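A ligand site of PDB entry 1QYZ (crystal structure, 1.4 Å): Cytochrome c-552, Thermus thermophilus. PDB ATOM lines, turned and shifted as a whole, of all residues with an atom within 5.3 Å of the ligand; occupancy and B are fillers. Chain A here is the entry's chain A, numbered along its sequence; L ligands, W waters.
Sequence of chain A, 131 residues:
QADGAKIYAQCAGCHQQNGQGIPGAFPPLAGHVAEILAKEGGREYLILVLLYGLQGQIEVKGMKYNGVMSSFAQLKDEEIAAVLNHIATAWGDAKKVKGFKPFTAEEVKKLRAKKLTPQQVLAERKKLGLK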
ATOM      1  N   ILE A   7      19.447 -17.427  -9.752  1.00  0.00           N
ATOM      2  CA  ILE A   7      18.481 -17.052  -8.722  1.00  0.00           C
ATOM      3  C   ILE A   7      17.196 -16.540  -9.373  1.00  0.00           C
ATOM      4  O   ILE A   7      16.085 -16.951  -9.012  1.00  0.00           O
ATOM      5  CB  ILE A   7      19.059 -16.006  -7.762  1.00  0.00           C
ATOM      6  CG1 ILE A   7      20.322 -16.491  -7.073  1.00  0.00           C
ATOM      7  CG2 ILE A   7      17.947 -15.588  -6.811  1.00  0.00           C
ATOM      8  CD1 ILE A   7      21.262 -15.458  -6.485  1.00  0.00           C
ATOM      9  N   TYR A   8      17.340 -15.655 -10.350  1.00  0.00           N
ATOM     10  CA  TYR A   8      16.173 -15.132 -11.047  1.00  0.00           C
ATOM     11  C   TYR A   8      15.323 -16.244 -11.651  1.00  0.00           C
ATOM     12  O   TYR A   8      14.090 -16.198 -11.575  1.00  0.00           O
ATOM     13  CB  TYR A   8      16.567 -14.117 -12.161  1.00  0.00           C
ATOM     14  CG  TYR A   8      15.295 -13.539 -12.763  1.00  0.00           C
ATOM     15  CD1 TYR A   8      14.818 -13.946 -14.007  1.00  0.00           C
ATOM     16  CD2 TYR A   8      14.563 -12.561 -12.063  1.00  0.00           C
ATOM     17  CE1 TYR A   8      13.664 -13.414 -14.543  1.00  0.00           C
ATOM     18  CE2 TYR A   8      13.410 -12.041 -12.611  1.00  0.00           C
ATOM     19  CZ  TYR A   8      12.962 -12.466 -13.844  1.00  0.00           C
ATOM     20  OH  TYR A   8      11.801 -11.938 -14.384  1.00  0.00           O
ATOM     21  N   CYS A  11      12.893 -17.845  -9.525  1.00  0.00           N
ATOM     22  CA  CYS A  11      11.642 -17.062  -9.023  1.00  0.00           C
ATOM     23  C   CYS A  11      10.954 -16.215 -10.026  1.00  0.00           C
ATOM     24  O   CYS A  11      10.268 -15.271 -10.015  1.00  0.00           O
ATOM     25  CB  CYS A  11      12.116 -16.237  -7.887  1.00  0.00           C
ATOM     26  SG  CYS A  11      13.407 -14.882  -8.332  1.00  0.00           S
ATOM     27  N   ALA A  12      11.115 -16.637 -11.347  1.00  0.00           N
ATOM     28  CA  ALA A  12      10.692 -15.940 -12.553  1.00  0.00           C
ATOM     29  C   ALA A  12       9.264 -16.273 -12.957  1.00  0.00           C
ATOM     30  O   ALA A  12       8.829 -15.866 -14.045  1.00  0.00           O
ATOM     31  CB  ALA A  12      11.623 -16.289 -13.716  1.00  0.00           C
ATOM     32  N   CYS A  14       6.404 -15.202 -12.277  1.00  0.00           N
ATOM     33  CA  CYS A  14       5.502 -14.061 -12.354  1.00  0.00           C
ATOM     34  C   CYS A  14       5.962 -13.076 -13.421  1.00  0.00           C
ATOM     35  O   CYS A  14       5.252 -12.859 -14.402  1.00  0.00           O
ATOM     36  CB  CYS A  14       5.347 -13.384 -10.983  1.00  0.00           C
ATOM     37  SG  CYS A  14       4.581 -14.518  -9.795  1.00  0.00           S
ATOM     38  N   HIS A  15       7.179 -12.500 -13.262  1.00  0.00           N
ATOM     39  CA  HIS A  15       7.677 -11.506 -14.191  1.00  0.00           C
ATOM     40  C   HIS A  15       8.218 -12.146 -15.475  1.00  0.00           C
ATOM     41  O   HIS A  15       8.498 -11.426 -16.439  1.00  0.00           O
ATOM     42  CB  HIS A  15       8.770 -10.638 -13.549  1.00  0.00           C
ATOM     43  CG  HIS A  15       8.298  -9.932 -12.301  1.00  0.00           C
ATOM     44  ND1 HIS A  15       7.472  -8.837 -12.329  1.00  0.00           N
ATOM     45  CD2 HIS A  15       8.521 -10.170 -10.985  1.00  0.00           C
ATOM     46  CE1 HIS A  15       7.212  -8.417 -11.085  1.00  0.00           C
ATOM     47  NE2 HIS A  15       7.852  -9.222 -10.228  1.00  0.00           N
ATOM     48  N   ALA A  25      -1.307  -8.249 -14.520  1.00  0.00           N
ATOM     49  CA  ALA A  25      -1.101  -9.155 -13.394  1.00  0.00           C
ATOM     50  C   ALA A  25       0.262  -8.947 -12.728  1.00  0.00           C
ATOM     51  O   ALA A  25       0.296  -8.672 -11.531  1.00  0.00           O
ATOM     52  CB  ALA A  25      -1.248 -10.612 -13.840  1.00  0.00           C
ATOM     53  N   PHE A  26       1.318  -9.131 -13.505  1.00  0.00           N
ATOM     54  CA  PHE A  26       2.694  -9.032 -13.014  1.00  0.00           C
ATOM     55  C   PHE A  26       3.426  -7.976 -13.832  1.00  0.00           C
ATOM     56  O   PHE A  26       3.562  -8.075 -15.063  1.00  0.00           O
ATOM     57  CB  PHE A  26       3.411 -10.381 -13.059  1.00  0.00           C
ATOM     58  CG  PHE A  26       2.578 -11.510 -12.481  1.00  0.00           C
ATOM     59  CD1 PHE A  26       2.154 -11.428 -11.159  1.00  0.00           C
ATOM     60  CD2 PHE A  26       2.218 -12.628 -13.225  1.00  0.00           C
ATOM     61  CE1 PHE A  26       1.387 -12.421 -10.588  1.00  0.00           C
ATOM     62  CE2 PHE A  26       1.443 -13.626 -12.659  1.00  0.00           C
ATOM     63  CZ  PHE A  26       1.030 -13.516 -11.338  1.00  0.00           C
ATOM     64  N   PRO A  27       3.910  -6.894 -13.216  1.00  0.00           N
ATOM     65  CA  PRO A  27       4.445  -5.818 -14.062  1.00  0.00           C
ATOM     66  C   PRO A  27       5.742  -6.208 -14.741  1.00  0.00           C
ATOM     67  O   PRO A  27       6.504  -7.051 -14.277  1.00  0.00           O
ATOM     68  CB  PRO A  27       4.637  -4.665 -13.078  1.00  0.00           C
ATOM     69  CG  PRO A  27       4.743  -5.290 -11.747  1.00  0.00           C
ATOM     70  CD  PRO A  27       3.985  -6.590 -11.788  1.00  0.00           C
ATOM     71  N   LEU A  29       9.579  -6.014 -15.817  1.00  0.00           N
ATOM     72  CA  LEU A  29      10.883  -5.571 -15.342  1.00  0.00           C
ATOM     73  C   LEU A  29      11.753  -5.045 -16.484  1.00  0.00           C
ATOM     74  O   LEU A  29      12.364  -3.978 -16.418  1.00  0.00           O
ATOM     75  CB  LEU A  29      11.619  -6.733 -14.626  1.00  0.00           C
ATOM     76  CG  LEU A  29      10.833  -7.289 -13.420  1.00  0.00           C
ATOM     77  CD1 LEU A  29      11.646  -8.356 -12.712  1.00  0.00           C
ATOM     78  CD2 LEU A  29      10.429  -6.155 -12.478  1.00  0.00           C
ATOM     79  N   HIS A  32      11.673  -1.389 -17.506  1.00  0.00           N
ATOM     80  CA  HIS A  32      11.041  -0.622 -16.429  1.00  0.00           C
ATOM     81  C   HIS A  32      12.006  -0.408 -15.265  1.00  0.00           C
ATOM     82  O   HIS A  32      11.928   0.575 -14.500  1.00  0.00           O
ATOM     83  CB  HIS A  32       9.764  -1.360 -16.000  1.00  0.00           C
ATOM     84  CG  HIS A  32       9.087  -0.786 -14.795  1.00  0.00           C
ATOM     85  ND1 HIS A  32       8.756   0.543 -14.673  1.00  0.00           N
ATOM     86  CD2 HIS A  32       8.682  -1.376 -13.658  1.00  0.00           C
ATOM     87  CE1 HIS A  32       8.167   0.765 -13.501  1.00  0.00           C
ATOM     88  NE2 HIS A  32       8.106  -0.400 -12.868  1.00  0.00           N
ATOM     89  N   ILE A  36      12.918   3.136 -12.816  1.00  0.00           N
ATOM     90  CA  ILE A  36      13.020   3.254 -11.358  1.00  0.00           C
ATOM     91  C   ILE A  36      14.415   3.737 -10.981  1.00  0.00           C
ATOM     92  O   ILE A  36      14.571   4.632 -10.159  1.00  0.00           O
ATOM     93  CB  ILE A  36      12.686   1.917 -10.692  1.00  0.00           C
ATOM     94  CG1 ILE A  36      11.216   1.501 -10.874  1.00  0.00           C
ATOM     95  CG2 ILE A  36      13.073   1.913  -9.216  1.00  0.00           C
ATOM     96  CD1 ILE A  36      10.981   0.038 -10.579  1.00  0.00           C
ATOM     97  N   TYR A  45      14.936   1.541  -3.292  1.00  0.00           N
ATOM     98  CA  TYR A  45      13.573   1.025  -3.452  1.00  0.00           C
ATOM     99  C   TYR A  45      13.603  -0.393  -3.992  1.00  0.00           C
ATOM    100  O   TYR A  45      12.866  -1.250  -3.455  1.00  0.00           O
ATOM    101  CB  TYR A  45      12.752   1.995  -4.331  1.00  0.00           C
ATOM    102  CG  TYR A  45      11.430   1.325  -4.693  1.00  0.00           C
ATOM    103  CD1 TYR A  45      10.432   1.148  -3.733  1.00  0.00           C
ATOM    104  CD2 TYR A  45      11.224   0.885  -5.988  1.00  0.00           C
ATOM    105  CE1 TYR A  45       9.225   0.541  -4.046  1.00  0.00           C
ATOM    106  CE2 TYR A  45      10.033   0.275  -6.306  1.00  0.00           C
ATOM    107  CZ  TYR A  45       9.044   0.090  -5.354  1.00  0.00           C
ATOM    108  OH  TYR A  45       7.849  -0.521  -5.663  1.00  0.00           O
ATOM    109  N   LEU A  46      14.405  -0.672  -5.002  1.00  0.00           N
ATOM    110  CA  LEU A  46      14.468  -2.030  -5.574  1.00  0.00           C
ATOM    111  C   LEU A  46      14.908  -3.036  -4.526  1.00  0.00           C
ATOM    112  O   LEU A  46      14.415  -4.155  -4.448  1.00  0.00           O
ATOM    113  CB  LEU A  46      15.390  -2.073  -6.807  1.00  0.00           C
ATOM    114  CG  LEU A  46      14.884  -1.285  -8.026  1.00  0.00           C
ATOM    115  CD1 LEU A  46      16.011  -1.103  -9.050  1.00  0.00           C
ATOM    116  CD2 LEU A  46      13.716  -1.991  -8.700  1.00  0.00           C
ATOM    117  N   VAL A  49      11.967  -3.739  -2.121  1.00  0.00           N
ATOM    118  CA  VAL A  49      10.947  -4.641  -2.670  1.00  0.00           C
ATOM    119  C   VAL A  49      11.380  -6.079  -2.433  1.00  0.00           C
ATOM    120  O   VAL A  49      10.592  -6.928  -2.027  1.00  0.00           O
ATOM    121  CB  VAL A  49      10.697  -4.397  -4.162  1.00  0.00           C
ATOM    122  CG1 VAL A  49       9.770  -5.439  -4.790  1.00  0.00           C
ATOM    123  CG2 VAL A  49      10.098  -2.998  -4.378  1.00  0.00           C
ATOM    124  N   LEU A  50      12.670  -6.368  -2.672  1.00  0.00           N
ATOM    125  CA  LEU A  50      13.125  -7.758  -2.529  1.00  0.00           C
ATOM    126  C   LEU A  50      13.182  -8.159  -1.054  1.00  0.00           C
ATOM    127  O   LEU A  50      12.898  -9.328  -0.717  1.00  0.00           O
ATOM    128  CB  LEU A  50      14.496  -7.951  -3.203  1.00  0.00           C
ATOM    129  CG  LEU A  50      14.467  -8.337  -4.678  1.00  0.00           C
ATOM    130  CD1 LEU A  50      13.995  -9.790  -4.814  1.00  0.00           C
ATOM    131  CD2 LEU A  50      13.574  -7.385  -5.447  1.00  0.00           C
ATOM    132  N   LEU A  54       5.783  -5.971  -1.562  1.00  0.00           N
ATOM    133  CA  LEU A  54       5.080  -4.808  -2.076  1.00  0.00           C
ATOM    134  C   LEU A  54       3.593  -5.135  -2.175  1.00  0.00           C
ATOM    135  O   LEU A  54       3.225  -6.270  -2.397  1.00  0.00           O
ATOM    136  CB  LEU A  54       5.629  -4.412  -3.453  1.00  0.00           C
ATOM    137  CG  LEU A  54       5.059  -3.160  -4.127  1.00  0.00           C
ATOM    138  CD1 LEU A  54       5.327  -1.913  -3.295  1.00  0.00           C
ATOM    139  CD2 LEU A  54       5.616  -2.989  -5.543  1.00  0.00           C
ATOM    140  N   GLN A  55       2.773  -4.118  -1.958  1.00  0.00           N
ATOM    141  CA  GLN A  55       1.334  -4.218  -2.202  1.00  0.00           C
ATOM    142  C   GLN A  55       0.837  -2.847  -2.586  1.00  0.00           C
ATOM    143  O   GLN A  55       1.563  -1.841  -2.480  1.00  0.00           O
ATOM    144  CB  GLN A  55       0.612  -4.748  -0.952  1.00  0.00           C
ATOM    145  CG  GLN A  55       0.619  -3.713   0.176  1.00  0.00           C
ATOM    146  CD  GLN A  55       0.139  -4.317   1.476  1.00  0.00           C
ATOM    147  OE1 GLN A  55       0.420  -5.505   1.738  1.00  0.00           O
ATOM    148  NE2 GLN A  55      -0.567  -3.510   2.263  1.00  0.00           N
ATOM    149  N   GLY A  56      -0.394  -2.756  -3.053  1.00  0.00           N
ATOM    150  CA  GLY A  56      -0.994  -1.491  -3.387  1.00  0.00           C
ATOM    151  C   GLY A  56      -1.154  -1.222  -4.859  1.00  0.00           C
ATOM    152  O   GLY A  56      -0.493  -1.831  -5.702  1.00  0.00           O
ATOM    153  N   GLN A  57      -2.031  -0.283  -5.205  1.00  0.00           N
ATOM    154  CA  GLN A  57      -2.208   0.073  -6.617  1.00  0.00           C
ATOM    155  C   GLN A  57      -1.013   0.863  -7.140  1.00  0.00           C
ATOM    156  O   GLN A  57      -0.630   1.849  -6.493  1.00  0.00           O
ATOM    157  CB  GLN A  57      -3.482   0.889  -6.791  1.00  0.00           C
ATOM    158  CG  GLN A  57      -3.552   1.611  -8.126  1.00  0.00           C
ATOM    159  CD  GLN A  57      -4.945   1.887  -8.626  1.00  0.00           C
ATOM    160  OE1 GLN A  57      -5.847   1.073  -8.452  1.00  0.00           O
ATOM    161  NE2 GLN A  57      -5.116   3.044  -9.262  1.00  0.00           N
ATOM    162  N   ILE A  58      -0.458   0.436  -8.268  1.00  0.00           N
ATOM    163  CA  ILE A  58       0.644   1.121  -8.935  1.00  0.00           C
ATOM    164  C   ILE A  58       0.384   1.189 -10.434  1.00  0.00           C
ATOM    165  O   ILE A  58      -0.461   0.449 -10.940  1.00  0.00           O
ATOM    166  CB  ILE A  58       1.998   0.420  -8.677  1.00  0.00           C
ATOM    167  CG1 ILE A  58       2.077  -0.939  -9.352  1.00  0.00           C
ATOM    168  CG2 ILE A  58       2.276   0.385  -7.175  1.00  0.00           C
ATOM    169  CD1 ILE A  58       3.352  -1.722  -9.195  1.00  0.00           C
ATOM    170  N   GLU A  59       1.108   2.059 -11.129  1.00  0.00           N
ATOM    171  CA  GLU A  59       1.048   2.145 -12.572  1.00  0.00           C
ATOM    172  C   GLU A  59       2.426   1.839 -13.160  1.00  0.00           C
ATOM    173  O   GLU A  59       3.442   2.307 -12.641  1.00  0.00           O
ATOM    174  CB  GLU A  59       0.603   3.524 -13.042  1.00  0.00           C
ATOM    175  CG  GLU A  59       0.216   3.529 -14.518  1.00  0.00           C
ATOM    176  CD  GLU A  59      -0.615   4.765 -14.836  1.00  0.00           C
ATOM    177  OE1 GLU A  59      -1.389   5.195 -13.946  1.00  0.00           O
ATOM    178  OE2 GLU A  59      -0.473   5.298 -15.963  1.00  0.00           O
ATOM    179  N   VAL A  60       2.460   1.023 -14.218  1.00  0.00           N
ATOM    180  CA  VAL A  60       3.672   0.675 -14.950  1.00  0.00           C
ATOM    181  C   VAL A  60       3.383   0.673 -16.439  1.00  0.00           C
ATOM    182  O   VAL A  60       2.538  -0.067 -16.944  1.00  0.00           O
ATOM    183  CB  VAL A  60       4.262  -0.678 -14.523  1.00  0.00           C
ATOM    184  CG1 VAL A  60       5.560  -0.960 -15.274  1.00  0.00           C
ATOM    185  CG2 VAL A  60       4.504  -0.720 -13.016  1.00  0.00           C
ATOM    186  N   TYR A  65      -1.727  -1.912 -11.890  1.00  0.00           N
ATOM    187  CA  TYR A  65      -1.555  -3.138 -11.132  1.00  0.00           C
ATOM    188  C   TYR A  65      -2.069  -2.969  -9.704  1.00  0.00           C
ATOM    189  O   TYR A  65      -1.985  -1.906  -9.121  1.00  0.00           O
ATOM    190  CB  TYR A  65      -0.086  -3.593 -11.097  1.00  0.00           C
ATOM    191  CG  TYR A  65       0.410  -3.860 -12.503  1.00  0.00           C
ATOM    192  CD1 TYR A  65       0.848  -2.808 -13.307  1.00  0.00           C
ATOM    193  CD2 TYR A  65       0.392  -5.156 -13.035  1.00  0.00           C
ATOM    194  CE1 TYR A  65       1.274  -3.056 -14.597  1.00  0.00           C
ATOM    195  CE2 TYR A  65       0.838  -5.394 -14.327  1.00  0.00           C
ATOM    196  CZ  TYR A  65       1.268  -4.342 -15.090  1.00  0.00           C
ATOM    197  OH  TYR A  65       1.701  -4.564 -16.374  1.00  0.00           O
ATOM    198  N   ASN A  66      -2.632  -4.027  -9.142  1.00  0.00           N
ATOM    199  CA  ASN A  66      -3.116  -3.960  -7.760  1.00  0.00           C
ATOM    200  C   ASN A  66      -2.936  -5.354  -7.176  1.00  0.00           C
ATOM    201  O   ASN A  66      -3.924  -6.005  -6.818  1.00  0.00           O
ATOM    202  CB  ASN A  66      -4.567  -3.528  -7.658  1.00  0.00           C
ATOM    203  CG  ASN A  66      -4.954  -3.148  -6.244  1.00  0.00           C
ATOM    204  OD1 ASN A  66      -4.116  -2.945  -5.357  1.00  0.00           O
ATOM    205  ND2 ASN A  66      -6.258  -3.048  -6.016  1.00  0.00           N
ATOM    206  N   GLY A  67      -1.674  -5.758  -7.136  1.00  0.00           N
ATOM    207  CA  GLY A  67      -1.355  -7.098  -6.637  1.00  0.00           C
ATOM    208  C   GLY A  67      -0.481  -7.062  -5.395  1.00  0.00           C
ATOM    209  O   GLY A  67      -0.334  -6.029  -4.755  1.00  0.00           O
ATOM    210  N   VAL A  68       0.069  -8.229  -5.069  1.00  0.00           N
ATOM    211  CA  VAL A  68       0.951  -8.433  -3.923  1.00  0.00           C
ATOM    212  C   VAL A  68       2.204  -9.185  -4.342  1.00  0.00           C
ATOM    213  O   VAL A  68       2.136 -10.113  -5.152  1.00  0.00           O
ATOM    214  CB  VAL A  68       0.286  -9.189  -2.757  1.00  0.00           C
ATOM    215  CG1 VAL A  68       1.282  -9.530  -1.658  1.00  0.00           C
ATOM    216  CG2 VAL A  68      -0.864  -8.371  -2.195  1.00  0.00           C
ATOM    217  N   MET A  69       3.323  -8.787  -3.800  1.00  0.00           N
ATOM    218  CA  MET A  69       4.563  -9.557  -3.953  1.00  0.00           C
ATOM    219  C   MET A  69       5.108  -9.847  -2.548  1.00  0.00           C
ATOM    220  O   MET A  69       5.125  -8.943  -1.709  1.00  0.00           O
ATOM    221  CB  MET A  69       5.569  -8.790  -4.793  1.00  0.00           C
ATOM    222  CG  MET A  69       6.897  -9.539  -4.970  1.00  0.00           C
ATOM    223  SD  MET A  69       8.071  -8.573  -5.962  1.00  0.00           S
ATOM    224  CE  MET A  69       9.597  -9.154  -5.216  1.00  0.00           C
ATOM    225  N   PHE A  72      11.459 -11.610  -0.171  1.00  0.00           N
ATOM    226  CA  PHE A  72      12.497 -12.591  -0.508  1.00  0.00           C
ATOM    227  C   PHE A  72      13.714 -12.438   0.405  1.00  0.00           C
ATOM    228  O   PHE A  72      14.868 -12.664  -0.005  1.00  0.00           O
ATOM    229  CB  PHE A  72      12.898 -12.426  -1.981  1.00  0.00           C
ATOM    230  CG  PHE A  72      11.851 -13.056  -2.899  1.00  0.00           C
ATOM    231  CD1 PHE A  72      10.683 -12.377  -3.201  1.00  0.00           C
ATOM    232  CD2 PHE A  72      12.069 -14.310  -3.445  1.00  0.00           C
ATOM    233  CE1 PHE A  72       9.723 -12.944  -4.039  1.00  0.00           C
ATOM    234  CE2 PHE A  72      11.114 -14.885  -4.260  1.00  0.00           C
ATOM    235  CZ  PHE A  72       9.945 -14.205  -4.561  1.00  0.00           C
ATOM    236  N   VAL A  83      20.594 -10.842  -7.924  1.00  0.00           N
ATOM    237  CA  VAL A  83      19.382 -10.863  -8.772  1.00  0.00           C
ATOM    238  C   VAL A  83      19.035  -9.456  -9.240  1.00  0.00           C
ATOM    239  O   VAL A  83      18.486  -9.289 -10.334  1.00  0.00           O
ATOM    240  CB  VAL A  83      18.265 -11.556  -7.970  1.00  0.00           C
ATOM    241  CG1 VAL A  83      17.693 -10.688  -6.875  1.00  0.00           C
ATOM    242  CG2 VAL A  83      17.187 -11.994  -8.962  1.00  0.00           C
ATOM    243  N   LEU A  84      19.326  -8.415  -8.449  1.00  0.00           N
ATOM    244  CA  LEU A  84      19.069  -7.027  -8.902  1.00  0.00           C
ATOM    245  C   LEU A  84      20.016  -6.688 -10.037  1.00  0.00           C
ATOM    246  O   LEU A  84      19.575  -6.025 -11.003  1.00  0.00           O
ATOM    247  CB  LEU A  84      19.162  -6.036  -7.743  1.00  0.00           C
ATOM    248  CG  LEU A  84      18.002  -6.234  -6.713  1.00  0.00           C
ATOM    249  CD1 LEU A  84      18.228  -5.361  -5.491  1.00  0.00           C
ATOM    250  CD2 LEU A  84      16.661  -5.956  -7.367  1.00  0.00           C
ATOM    251  N   ILE A  87      18.363  -8.257 -13.177  1.00  0.00           N
ATOM    252  CA  ILE A  87      17.200  -7.577 -13.783  1.00  0.00           C
ATOM    253  C   ILE A  87      17.632  -6.211 -14.304  1.00  0.00           C
ATOM    254  O   ILE A  87      16.957  -5.676 -15.214  1.00  0.00           O
ATOM    255  CB  ILE A  87      15.994  -7.457 -12.839  1.00  0.00           C
ATOM    256  CG1 ILE A  87      16.160  -6.460 -11.658  1.00  0.00           C
ATOM    257  CG2 ILE A  87      15.588  -8.834 -12.331  1.00  0.00           C
ATOM    258  CD1 ILE A  87      14.875  -6.267 -10.837  1.00  0.00           C
ATOM    259  N   ARG A 125       7.825   3.822  -2.727  1.00  0.00           N
ATOM    260  CA  ARG A 125       7.650   3.983  -4.176  1.00  0.00           C
ATOM    261  C   ARG A 125       7.072   5.361  -4.507  1.00  0.00           C
ATOM    262  O   ARG A 125       7.512   5.995  -5.468  1.00  0.00           O
ATOM    263  CB  ARG A 125       6.721   2.892  -4.723  1.00  0.00           C
ATOM    264  CG  ARG A 125       6.684   2.780  -6.240  1.00  0.00           C
ATOM    265  CD  ARG A 125       5.663   1.752  -6.676  1.00  0.00           C
ATOM    266  NE  ARG A 125       5.769   1.363  -8.070  1.00  0.00           N
ATOM    267  CZ  ARG A 125       5.182   2.002  -9.092  1.00  0.00           C
ATOM    268  NH1 ARG A 125       4.445   3.078  -8.809  1.00  0.00           N
ATOM    269  NH2 ARG A 125       5.366   1.553 -10.329  1.00  0.00           N
HETATM  270 FE1  LIG L   1       7.945  -9.020  -8.235  1.00  0.00          FE
HETATM  271  C1  LIG L   1       6.624  -5.862  -8.207  1.00  0.00           C
HETATM  272  C2  LIG L   1      11.047  -7.734  -8.706  1.00  0.00           C
HETATM  273  C3  LIG L   1       9.216 -12.104  -7.757  1.00  0.00           C
HETATM  274  C4  LIG L   1       4.781 -10.289  -8.272  1.00  0.00           C
HETATM  275  N1  LIG L   1       8.679  -7.177  -8.446  1.00  0.00           N
HETATM  276  N2  LIG L   1       9.784  -9.810  -8.285  1.00  0.00           N
HETATM  277  N3  LIG L   1       7.128 -10.842  -7.958  1.00  0.00           N
HETATM  278  N4  LIG L   1       6.052  -8.228  -8.252  1.00  0.00           N
HETATM  279  C5  LIG L   1       7.989  -5.936  -8.361  1.00  0.00           C
HETATM  280  C6  LIG L   1       8.891  -4.898  -8.437  1.00  0.00           C
HETATM  281  C7  LIG L   1      10.152  -5.397  -8.708  1.00  0.00           C
HETATM  282  C8  LIG L   1       9.989  -6.794  -8.603  1.00  0.00           C
HETATM  283  C9  LIG L   1      11.452  -4.661  -8.765  1.00  0.00           C
HETATM  284  C10 LIG L   1       8.576  -3.352  -8.388  1.00  0.00           C
HETATM  285  C11 LIG L   1       8.021  -2.800  -9.694  1.00  0.00           C
HETATM  286  C12 LIG L   1       7.481  -1.367  -9.473  1.00  0.00           C
HETATM  287  O1  LIG L   1       7.064  -0.773 -10.460  1.00  0.00           O
HETATM  288  O2  LIG L   1       7.363  -0.869  -8.321  1.00  0.00           O
HETATM  289  C13 LIG L   1      10.951  -9.132  -8.484  1.00  0.00           C
HETATM  290  C14 LIG L   1      12.061 -10.057  -8.463  1.00  0.00           C
HETATM  291  C15 LIG L   1      11.541 -11.240  -8.043  1.00  0.00           C
HETATM  292  C16 LIG L   1      10.160 -11.106  -8.019  1.00  0.00           C
HETATM  293  C17 LIG L   1      13.535  -9.627  -8.817  1.00  0.00           C
HETATM  294  C18 LIG L   1      12.334 -12.536  -7.926  1.00  0.00           C
HETATM  295  C19 LIG L   1      12.889 -13.128  -9.264  1.00  0.00           C
HETATM  296  O3  LIG L   1      11.921 -13.092  -6.612  1.00  0.00           O
HETATM  297  C20 LIG L   1       7.838 -12.033  -7.818  1.00  0.00           C
HETATM  298  C21 LIG L   1       6.885 -13.122  -7.782  1.00  0.00           C
HETATM  299  C22 LIG L   1       5.712 -12.674  -8.118  1.00  0.00           C
HETATM  300  C23 LIG L   1       5.806 -11.284  -8.155  1.00  0.00           C
HETATM  301  C24 LIG L   1       7.415 -14.545  -7.556  1.00  0.00           C
HETATM  302  C25 LIG L   1       4.384 -13.380  -8.333  1.00  0.00           C
HETATM  303  C26 LIG L   1       3.930 -14.235  -7.102  1.00  0.00           C
HETATM  304  C27 LIG L   1       4.848  -8.925  -8.303  1.00  0.00           C
HETATM  305  C28 LIG L   1       3.707  -8.038  -8.321  1.00  0.00           C
HETATM  306  C29 LIG L   1       4.263  -6.775  -8.142  1.00  0.00           C
HETATM  307  C30 LIG L   1       5.670  -6.927  -8.146  1.00  0.00           C
HETATM  308  C31 LIG L   1       2.266  -8.522  -8.290  1.00  0.00           C
HETATM  309  C32 LIG L   1       3.471  -5.460  -8.035  1.00  0.00           C
HETATM  310  C33 LIG L   1       2.760  -5.374  -6.650  1.00  0.00           C
HETATM  311  C34 LIG L   1       1.540  -4.534  -6.610  1.00  0.00           C
HETATM  312  O4  LIG L   1       1.575  -3.559  -5.687  1.00  0.00           O
HETATM  313  O5  LIG L   1       0.848  -4.425  -7.632  1.00  0.00           O
HETATM  314  O   HOH W   1       5.793 -12.931  -4.524  1.00  0.00           O
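Tyr 8 touches the ligand (CD2 to C19, 3.3 Å). Ala 25 touches the ligand. CE1 of Phe 26 touches C25 of the ligand, 3.9 Å away. CD of Pro 27 touches C29 of the ligand (3.7 Å). Leu 29 touches the ligand (CD2 to C7, 3.9 Å). CD1 of Ile 36 touches C12 of the ligand, at 3.9 Å. Leu 46 touches the ligand (CD2 to C9, 3.5 Å). CG1 of Val 49 touches C6 of the ligand, at 3.8 Å. Leu 54 touches the ligand (CG to O4, 3.8 Å). C of Gln 55 touches O4 of the ligand, at 3.3 Å. CD1 of Ile 58 touches C32 of the ligand, at 3.9 Å. Val 60 touches the ligand (CG2 to O1, 3.6 Å). Tyr 65 touches the ligand (CB to O5, 3.7 Å). Asn 66 touches the ligand (N to O5, 3.8 Å). Val 68 touches the ligand. Phe 72 touches the ligand. Hydrophobic or aromatic side chains within 4 Å of the ligand: Tyr 8, His 15, Phe 26, Pro 27, Leu 29, His 32, Ile 36, Tyr 45, Leu 46, Val 49, Leu 54, Ile 58, Val 60, Tyr 65, Met 69 and Phe 72. Along chain A the residues within 4 Å of the ligand span positions 8 to 125.
The backbone NH of Gly 56 lies within hydrogen-bond range of an oxygen (O4) of the ligand (3.4 Å). The side-chain sulfur (SG) of Cys 11 is covalently linked to a carbon (C19) of the ligand, 2.1 Å away. The backbone carbonyl oxygen (O) of Gly 56 lies close to an oxygen (O4) of the ligand, at 2.7 Å. NE2 of His 15 is bound to FE1 of the ligand (2.0 Å). A carbon (C25) of the ligand is covalently linked to the side-chain sulfur (SG) of Cys 14 (1.9 Å). The backbone NH (N) of Gly 67 lies within hydrogen-bond range of an oxygen (O5) of the ligand (2.9 Å). OH of Tyr 45 is in hydrogen-bond range of O2 of the ligand (2.7 Å). A ring nitrogen (NE2) of His 32 sits at hydrogen-bond distance from an oxygen (O1) of the ligand (2.7 Å). FE1 of the ligand is bound by SD of Met 69 (2.3 Å). The guanidinium group (NE) of Arg 125 is in salt-bridge range of an oxygen (O2) of the ligand.
O of Leu 50 is in hydrogen-bond range of N of Phe 72 (2.8 Å). The backbone carbonyl oxygen of Ile 58 lies within hydrogen-bond range of the backbone NH of Tyr 65 (2.8 Å). The backbone NH of Met 69 sits at hydrogen-bond distance from the backbone carbonyl oxygen of Leu 54, 2.9 Å away. The backbone carbonyl oxygen of Glu 59 is in hydrogen-bond range of the guanidinium group of Arg 125 (3.1 Å). O of Pro 27 sits at hydrogen-bond distance from ND1 of His 15. OD1 of Asn 66 is in hydrogen-bond range of N of Gln 57 (3.4 Å).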
